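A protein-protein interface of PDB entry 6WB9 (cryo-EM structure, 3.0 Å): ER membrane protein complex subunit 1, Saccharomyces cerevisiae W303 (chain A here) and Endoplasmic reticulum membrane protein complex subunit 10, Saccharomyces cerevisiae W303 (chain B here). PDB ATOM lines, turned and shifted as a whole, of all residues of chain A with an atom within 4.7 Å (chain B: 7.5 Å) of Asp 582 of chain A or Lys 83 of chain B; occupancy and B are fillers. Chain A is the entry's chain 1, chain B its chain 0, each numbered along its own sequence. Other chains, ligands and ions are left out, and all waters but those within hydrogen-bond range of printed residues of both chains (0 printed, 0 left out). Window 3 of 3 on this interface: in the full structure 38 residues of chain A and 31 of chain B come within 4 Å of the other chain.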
ATOM      1  N   SER A 580      28.916  -5.552  37.723  1.00  0.00           N
ATOM      2  CA  SER A 580      29.975  -4.900  36.965  1.00  0.00           C
ATOM      3  C   SER A 580      29.328  -3.933  35.989  1.00  0.00           C
ATOM      4  O   SER A 580      28.484  -4.339  35.181  1.00  0.00           O
ATOM      5  CB  SER A 580      30.833  -5.924  36.218  1.00  0.00           C
ATOM      6  OG  SER A 580      30.053  -6.659  35.292  1.00  0.00           O
ATOM      7  N   TYR A 581      29.712  -2.664  36.067  1.00  0.00           N
ATOM      8  CA  TYR A 581      29.159  -1.665  35.165  1.00  0.00           C
ATOM      9  C   TYR A 581      29.723  -1.836  33.763  1.00  0.00           C
ATOM     10  O   TYR A 581      30.892  -2.182  33.580  1.00  0.00           O
ATOM     11  CB  TYR A 581      29.460  -0.257  35.671  1.00  0.00           C
ATOM     12  CG  TYR A 581      28.451   0.285  36.650  1.00  0.00           C
ATOM     13  CD1 TYR A 581      27.215   0.733  36.217  1.00  0.00           C
ATOM     14  CD2 TYR A 581      28.742   0.365  38.004  1.00  0.00           C
ATOM     15  CE1 TYR A 581      26.289   1.235  37.102  1.00  0.00           C
ATOM     16  CE2 TYR A 581      27.821   0.869  38.897  1.00  0.00           C
ATOM     17  CZ  TYR A 581      26.597   1.302  38.439  1.00  0.00           C
ATOM     18  OH  TYR A 581      25.674   1.803  39.323  1.00  0.00           O
ATOM     19  N   ASP A 582      28.873  -1.595  32.766  1.00  0.00           N
ATOM     20  CA  ASP A 582      29.261  -1.581  31.358  1.00  0.00           C
ATOM     21  C   ASP A 582      28.832  -0.232  30.802  1.00  0.00           C
ATOM     22  O   ASP A 582      27.672  -0.060  30.398  1.00  0.00           O
ATOM     23  CB  ASP A 582      28.618  -2.733  30.592  1.00  0.00           C
ATOM     24  CG  ASP A 582      29.118  -2.839  29.166  1.00  0.00           C
ATOM     25  OD1 ASP A 582      30.188  -2.276  28.861  1.00  0.00           O
ATOM     26  OD2 ASP A 582      28.434  -3.486  28.347  1.00  0.00           O
ATOM     27  N   PRO A 583      29.728   0.760  30.767  1.00  0.00           N
ATOM     28  CA  PRO A 583      29.325   2.098  30.322  1.00  0.00           C
ATOM     29  C   PRO A 583      29.168   2.233  28.820  1.00  0.00           C
ATOM     30  O   PRO A 583      28.690   3.277  28.363  1.00  0.00           O
ATOM     31  CB  PRO A 583      30.461   2.987  30.838  1.00  0.00           C
ATOM     32  CG  PRO A 583      31.632   2.103  30.865  1.00  0.00           C
ATOM     33  CD  PRO A 583      31.140   0.721  31.179  1.00  0.00           C
ATOM     34  N   LEU A 584      29.552   1.220  28.041  1.00  0.00           N
ATOM     35  CA  LEU A 584      29.269   1.229  26.611  1.00  0.00           C
ATOM     36  C   LEU A 584      27.795   0.981  26.331  1.00  0.00           C
ATOM     37  O   LEU A 584      27.294   1.391  25.280  1.00  0.00           O
ATOM     38  CB  LEU A 584      30.137   0.186  25.907  1.00  0.00           C
ATOM     39  CG  LEU A 584      30.226   0.213  24.381  1.00  0.00           C
ATOM     40  CD1 LEU A 584      30.490   1.618  23.883  1.00  0.00           C
ATOM     41  CD2 LEU A 584      31.307  -0.731  23.899  1.00  0.00           C
ATOM     42  N   THR A 585      27.088   0.330  27.252  1.00  0.00           N
ATOM     43  CA  THR A 585      25.641   0.213  27.156  1.00  0.00           C
ATOM     44  C   THR A 585      24.938   1.516  27.508  1.00  0.00           C
ATOM     45  O   THR A 585      23.814   1.746  27.055  1.00  0.00           O
ATOM     46  CB  THR A 585      25.144  -0.903  28.076  1.00  0.00           C
ATOM     47  OG1 THR A 585      25.725  -2.147  27.673  1.00  0.00           O
ATOM     48  CG2 THR A 585      23.633  -1.030  28.002  1.00  0.00           C
ATOM     49  N   GLY A 586      25.588   2.381  28.280  1.00  0.00           N
ATOM     50  CA  GLY A 586      24.972   3.574  28.808  1.00  0.00           C
ATOM     51  C   GLY A 586      24.378   3.399  30.183  1.00  0.00           C
ATOM     52  O   GLY A 586      23.976   4.391  30.800  1.00  0.00           O
ATOM     53  N   HIS A 587      24.327   2.167  30.688  1.00  0.00           N
ATOM     54  CA  HIS A 587      23.717   1.870  31.983  1.00  0.00           C
ATOM     55  C   HIS A 587      24.690   2.252  33.097  1.00  0.00           C
ATOM     56  O   HIS A 587      25.338   1.416  33.728  1.00  0.00           O
ATOM     57  CB  HIS A 587      23.319   0.403  32.059  1.00  0.00           C
ATOM     58  CG  HIS A 587      22.556   0.046  33.297  1.00  0.00           C
ATOM     59  ND1 HIS A 587      21.887   0.983  34.055  1.00  0.00           N
ATOM     60  CD2 HIS A 587      22.361  -1.143  33.912  1.00  0.00           C
ATOM     61  CE1 HIS A 587      21.311   0.384  35.082  1.00  0.00           C
ATOM     62  NE2 HIS A 587      21.585  -0.906  35.018  1.00  0.00           N
ATOM     63  N   VAL B  60      18.099  -5.675  17.449  1.00  0.00           N
ATOM     64  CA  VAL B  60      19.395  -5.017  17.363  1.00  0.00           C
ATOM     65  C   VAL B  60      20.192  -5.365  18.614  1.00  0.00           C
ATOM     66  O   VAL B  60      19.697  -5.213  19.736  1.00  0.00           O
ATOM     67  CB  VAL B  60      19.243  -3.488  17.189  1.00  0.00           C
ATOM     68  CG1 VAL B  60      18.558  -2.858  18.396  1.00  0.00           C
ATOM     69  CG2 VAL B  60      20.580  -2.826  16.921  1.00  0.00           C
ATOM     70  N   SER B  61      21.408  -5.872  18.419  1.00  0.00           N
ATOM     71  CA  SER B  61      22.292  -6.193  19.532  1.00  0.00           C
ATOM     72  C   SER B  61      23.729  -6.026  19.070  1.00  0.00           C
ATOM     73  O   SER B  61      24.115  -6.576  18.035  1.00  0.00           O
ATOM     74  CB  SER B  61      22.056  -7.618  20.037  1.00  0.00           C
ATOM     75  OG  SER B  61      22.362  -8.568  19.033  1.00  0.00           O
ATOM     76  N   GLY B  62      24.512  -5.270  19.830  1.00  0.00           N
ATOM     77  CA  GLY B  62      25.897  -5.014  19.499  1.00  0.00           C
ATOM     78  C   GLY B  62      26.214  -3.537  19.544  1.00  0.00           C
ATOM     79  O   GLY B  62      25.361  -2.696  19.809  1.00  0.00           O
ATOM     80  N   GLU B  63      27.480  -3.228  19.286  1.00  0.00           N
ATOM     81  CA  GLU B  63      27.968  -1.855  19.342  1.00  0.00           C
ATOM     82  C   GLU B  63      27.692  -1.169  18.010  1.00  0.00           C
ATOM     83  O   GLU B  63      28.197  -1.600  16.969  1.00  0.00           O
ATOM     84  CB  GLU B  63      29.459  -1.837  19.665  1.00  0.00           C
ATOM     85  CG  GLU B  63      29.813  -2.584  20.931  1.00  0.00           C
ATOM     86  CD  GLU B  63      31.282  -2.931  21.015  1.00  0.00           C
ATOM     87  OE1 GLU B  63      32.071  -2.384  20.216  1.00  0.00           O
ATOM     88  OE2 GLU B  63      31.646  -3.758  21.875  1.00  0.00           O
ATOM     89  N   TYR B  64      26.899  -0.100  18.045  1.00  0.00           N
ATOM     90  CA  TYR B  64      26.459   0.560  16.827  1.00  0.00           C
ATOM     91  C   TYR B  64      26.532   2.073  16.977  1.00  0.00           C
ATOM     92  O   TYR B  64      26.503   2.622  18.086  1.00  0.00           O
ATOM     93  CB  TYR B  64      25.031   0.153  16.445  1.00  0.00           C
ATOM     94  CG  TYR B  64      24.885  -1.302  16.068  1.00  0.00           C
ATOM     95  CD1 TYR B  64      25.434  -1.792  14.891  1.00  0.00           C
ATOM     96  CD2 TYR B  64      24.179  -2.179  16.878  1.00  0.00           C
ATOM     97  CE1 TYR B  64      25.299  -3.120  14.540  1.00  0.00           C
ATOM     98  CE2 TYR B  64      24.038  -3.508  16.538  1.00  0.00           C
ATOM     99  CZ  TYR B  64      24.598  -3.973  15.367  1.00  0.00           C
ATOM    100  OH  TYR B  64      24.457  -5.298  15.024  1.00  0.00           O
ATOM    101  N   LEU B  66      24.708   5.509  16.317  1.00  0.00           N
ATOM    102  CA  LEU B  66      23.346   6.010  16.187  1.00  0.00           C
ATOM    103  C   LEU B  66      23.357   7.360  15.486  1.00  0.00           C
ATOM    104  O   LEU B  66      24.187   8.214  15.798  1.00  0.00           O
ATOM    105  CB  LEU B  66      22.682   6.115  17.557  1.00  0.00           C
ATOM    106  CG  LEU B  66      22.061   4.793  17.997  1.00  0.00           C
ATOM    107  CD1 LEU B  66      23.125   3.749  18.227  1.00  0.00           C
ATOM    108  CD2 LEU B  66      21.222   4.991  19.242  1.00  0.00           C
ATOM    109  N   TYR B  81      27.596   6.080  20.357  1.00  0.00           N
ATOM    110  CA  TYR B  81      28.115   4.748  20.058  1.00  0.00           C
ATOM    111  C   TYR B  81      27.739   3.856  21.229  1.00  0.00           C
ATOM    112  O   TYR B  81      28.383   3.904  22.279  1.00  0.00           O
ATOM    113  CB  TYR B  81      29.619   4.772  19.858  1.00  0.00           C
ATOM    114  CG  TYR B  81      30.224   3.456  19.430  1.00  0.00           C
ATOM    115  CD1 TYR B  81      30.249   3.087  18.095  1.00  0.00           C
ATOM    116  CD2 TYR B  81      30.791   2.595  20.359  1.00  0.00           C
ATOM    117  CE1 TYR B  81      30.806   1.893  17.698  1.00  0.00           C
ATOM    118  CE2 TYR B  81      31.351   1.397  19.973  1.00  0.00           C
ATOM    119  CZ  TYR B  81      31.357   1.053  18.641  1.00  0.00           C
ATOM    120  OH  TYR B  81      31.916  -0.139  18.245  1.00  0.00           O
ATOM    121  N   MET B  82      26.713   3.034  21.057  1.00  0.00           N
ATOM    122  CA  MET B  82      26.192   2.292  22.191  1.00  0.00           C
ATOM    123  C   MET B  82      26.164   0.800  21.908  1.00  0.00           C
ATOM    124  O   MET B  82      26.063   0.362  20.761  1.00  0.00           O
ATOM    125  CB  MET B  82      24.787   2.766  22.576  1.00  0.00           C
ATOM    126  CG  MET B  82      24.707   4.229  22.946  1.00  0.00           C
ATOM    127  SD  MET B  82      23.198   4.638  23.818  1.00  0.00           S
ATOM    128  CE  MET B  82      23.820   4.775  25.484  1.00  0.00           C
ATOM    129  N   LYS B  83      26.251   0.024  22.984  1.00  0.00           N
ATOM    130  CA  LYS B  83      26.047  -1.421  22.930  1.00  0.00           C
ATOM    131  C   LYS B  83      24.554  -1.652  23.110  1.00  0.00           C
ATOM    132  O   LYS B  83      24.051  -1.797  24.224  1.00  0.00           O
ATOM    133  CB  LYS B  83      26.871  -2.129  23.996  1.00  0.00           C
ATOM    134  CG  LYS B  83      26.808  -3.641  23.930  1.00  0.00           C
ATOM    135  CD  LYS B  83      27.288  -4.277  25.223  1.00  0.00           C
ATOM    136  CE  LYS B  83      28.719  -4.776  25.116  1.00  0.00           C
ATOM    137  NZ  LYS B  83      29.710  -3.678  24.979  1.00  0.00           N
ATOM    138  N   LEU B  84      23.836  -1.674  21.993  1.00  0.00           N
ATOM    139  CA  LEU B  84      22.386  -1.769  22.014  1.00  0.00           C
ATOM    140  C   LEU B  84      21.932  -3.207  22.230  1.00  0.00           C
ATOM    141  O   LEU B  84      22.510  -4.150  21.679  1.00  0.00           O
ATOM    142  CB  LEU B  84      21.808  -1.236  20.704  1.00  0.00           C
ATOM    143  CG  LEU B  84      22.216   0.185  20.323  1.00  0.00           C
ATOM    144  CD1 LEU B  84      21.755   0.519  18.919  1.00  0.00           C
ATOM    145  CD2 LEU B  84      21.645   1.172  21.317  1.00  0.00           C
ATOM    146  N   ARG B  85      20.889  -3.358  23.041  1.00  0.00           N
ATOM    147  CA  ARG B  85      20.198  -4.614  23.274  1.00  0.00           C
ATOM    148  C   ARG B  85      18.798  -4.515  22.680  1.00  0.00           C
ATOM    149  O   ARG B  85      18.296  -3.421  22.423  1.00  0.00           O
ATOM    150  CB  ARG B  85      20.131  -4.925  24.776  1.00  0.00           C
ATOM    151  CG  ARG B  85      20.022  -6.401  25.120  1.00  0.00           C
ATOM    152  CD  ARG B  85      21.205  -7.182  24.581  1.00  0.00           C
ATOM    153  NE  ARG B  85      20.896  -8.602  24.442  1.00  0.00           N
ATOM    154  CZ  ARG B  85      21.057  -9.502  25.406  1.00  0.00           C
ATOM    155  NH1 ARG B  85      20.749 -10.773  25.185  1.00  0.00           N
ATOM    156  NH2 ARG B  85      21.527  -9.133  26.590  1.00  0.00           N
ATOM    157  N   THR B  86      18.170  -5.675  22.451  1.00  0.00           N
ATOM    158  CA  THR B  86      16.886  -5.747  21.757  1.00  0.00           C
ATOM    159  C   THR B  86      15.738  -5.117  22.562  1.00  0.00           C
ATOM    160  O   THR B  86      14.914  -4.418  21.958  1.00  0.00           O
ATOM    161  CB  THR B  86      16.572  -7.200  21.360  1.00  0.00           C
ATOM    162  OG1 THR B  86      17.719  -7.783  20.729  1.00  0.00           O
ATOM    163  CG2 THR B  86      15.390  -7.263  20.403  1.00  0.00           C
ATOM    164  N   LEU B  88      15.256  -2.115  23.836  1.00  0.00           N
ATOM    165  CA  LEU B  88      15.927  -0.819  23.844  1.00  0.00           C
ATOM    166  C   LEU B  88      15.331   0.098  24.900  1.00  0.00           C
ATOM    167  O   LEU B  88      14.380   0.833  24.628  1.00  0.00           O
ATOM    168  CB  LEU B  88      15.826  -0.156  22.469  1.00  0.00           C
ATOM    169  CG  LEU B  88      16.648  -0.734  21.319  1.00  0.00           C
ATOM    170  CD1 LEU B  88      16.042  -0.347  19.985  1.00  0.00           C
ATOM    171  CD2 LEU B  88      18.079  -0.253  21.401  1.00  0.00           C
ATOM    172  N   TYR B  90      16.038   2.984  26.186  1.00  0.00           N
ATOM    173  CA  TYR B  90      16.784   4.219  26.031  1.00  0.00           C
ATOM    174  C   TYR B  90      15.842   5.414  25.988  1.00  0.00           C
ATOM    175  O   TYR B  90      14.619   5.279  25.922  1.00  0.00           O
ATOM    176  CB  TYR B  90      17.661   4.173  24.777  1.00  0.00           C
ATOM    177  CG  TYR B  90      18.791   3.184  24.899  1.00  0.00           C
ATOM    178  CD1 TYR B  90      19.923   3.488  25.642  1.00  0.00           C
ATOM    179  CD2 TYR B  90      18.719   1.941  24.290  1.00  0.00           C
ATOM    180  CE1 TYR B  90      20.953   2.583  25.767  1.00  0.00           C
ATOM    181  CE2 TYR B  90      19.747   1.028  24.412  1.00  0.00           C
ATOM    182  CZ  TYR B  90      20.860   1.358  25.150  1.00  0.00           C
ATOM    183  OH  TYR B  90      21.888   0.454  25.273  1.00  0.00           O
ATOM    184  N   LEU B 107      21.583   9.787  23.537  1.00  0.00           N
ATOM    185  CA  LEU B 107      20.783   8.634  23.934  1.00  0.00           C
ATOM    186  C   LEU B 107      21.142   8.267  25.365  1.00  0.00           C
ATOM    187  O   LEU B 107      22.205   7.692  25.612  1.00  0.00           O
ATOM    188  CB  LEU B 107      21.023   7.449  23.001  1.00  0.00           C
ATOM    189  CG  LEU B 107      20.339   6.109  23.271  1.00  0.00           C
ATOM    190  CD1 LEU B 107      18.842   6.277  23.173  1.00  0.00           C
ATOM    191  CD2 LEU B 107      20.804   5.039  22.315  1.00  0.00           C
ATOM    192  N   TYR B 109      20.292   6.222  29.035  1.00  0.00           N
ATOM    193  CA  TYR B 109      19.700   4.969  29.471  1.00  0.00           C
ATOM    194  C   TYR B 109      18.631   5.253  30.515  1.00  0.00           C
ATOM    195  O   TYR B 109      18.783   6.149  31.351  1.00  0.00           O
ATOM    196  CB  TYR B 109      20.762   4.033  30.045  1.00  0.00           C
ATOM    197  CG  TYR B 109      20.307   2.600  30.193  1.00  0.00           C
ATOM    198  CD1 TYR B 109      20.379   1.718  29.124  1.00  0.00           C
ATOM    199  CD2 TYR B 109      19.812   2.127  31.403  1.00  0.00           C
ATOM    200  CE1 TYR B 109      19.966   0.408  29.249  1.00  0.00           C
ATOM    201  CE2 TYR B 109      19.396   0.816  31.537  1.00  0.00           C
ATOM    202  CZ  TYR B 109      19.476  -0.036  30.456  1.00  0.00           C
ATOM    203  OH  TYR B 109      19.065  -1.343  30.580  1.00  0.00           O
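O of Lys 83 of chain B sits at hydrogen-bond distance from OH of Tyr 90 of chain B (3.3 Å).
The side-chain carboxylate of Glu 63 of chain B is in salt-bridge range of the side-chain amino group of Lys 83 of chain B.
OD2 of Asp 582 of chain A lies within hydrogen-bond range of OG1 of Thr 585 of chain A.
The backbone carbonyl oxygen (O) of Met 82 of chain B is in hydrogen-bond range of the backbone NH (N) of Tyr 64 of chain B, at 2.9 Å.
The side-chain carboxylate of Glu 63 of chain B is in hydrogen-bond range of the side-chain hydroxyl of Tyr 81 of chain B, 3.0 Å away.
Among the printed residues, merely in contact across the chains: Gly 586 of chain A with Tyr 109 of chain B, Leu 584 of chain A with Met 82 of chain B, Thr 585 of chain A with Met 82 of chain B, Leu 584 of chain A with Tyr 81 of chain B, His 587 of chain A with Tyr 109 of chain B, Thr 585 of chain A with Lys 83 of chain B, Leu 584 of chain A with Glu 63 of chain B and Gly 586 of chain A with Met 82 of chain B.
Asp 582 of chain A touches just one residue of chain B: Lys 83.
Of chain A, only Asp 582 (3.4 Å), Leu 584 (2.9 Å) and Thr 585 (3.6 Å) come within 4 Å of Lys 83 of chain B.
Printed residues of chain A within 4 Å of Met 82 of chain B: Leu 584, Thr 585 and Gly 586.
Printed residues of chain A within 4 Å of Glu 63 of chain B: Leu 584 (3.6 Å).
Arg 85 of chain B touches none of the printed residues of chain A.
Leu 66 of chain B touches none of the printed residues of chain A.
The nearest residue of chain B that does not touch Asp 582 of chain A is Glu 63 of chain B (7.2 Å).
The nearest printed residue of chain A that does not touch Lys 83 of chain B is Gly 586 of chain A (5.8 Å).
The backbone NH (N) of Lys 83 of chain B sits at hydrogen-bond distance from the backbone carbonyl oxygen (O) of Leu 584 of chain A (2.9 Å).
The backbone carbonyl oxygen (O) of Thr 585 of chain A sits at hydrogen-bond distance from the side-chain hydroxyl (OH) of Tyr 90 of chain B, 2.9 Å away.
NZ of Lys 83 of chain B lies within salt-bridge range of OD2 of Asp 582 of chain A, 3.6 Å away.
Of the 8 printed residues of chain A, 5 touch a printed residue of chain B.
Hydrophobic or aromatic side chains of chain A within 4 Å of the printed part of chain B: Leu 584 and His 587.
Hydrophobic or aromatic side chains of chain B that line the printed part of chain A: Tyr 81, Met 82, Tyr 90 and Tyr 109.
Among the printed residues, 11 pairs touch across the chains.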
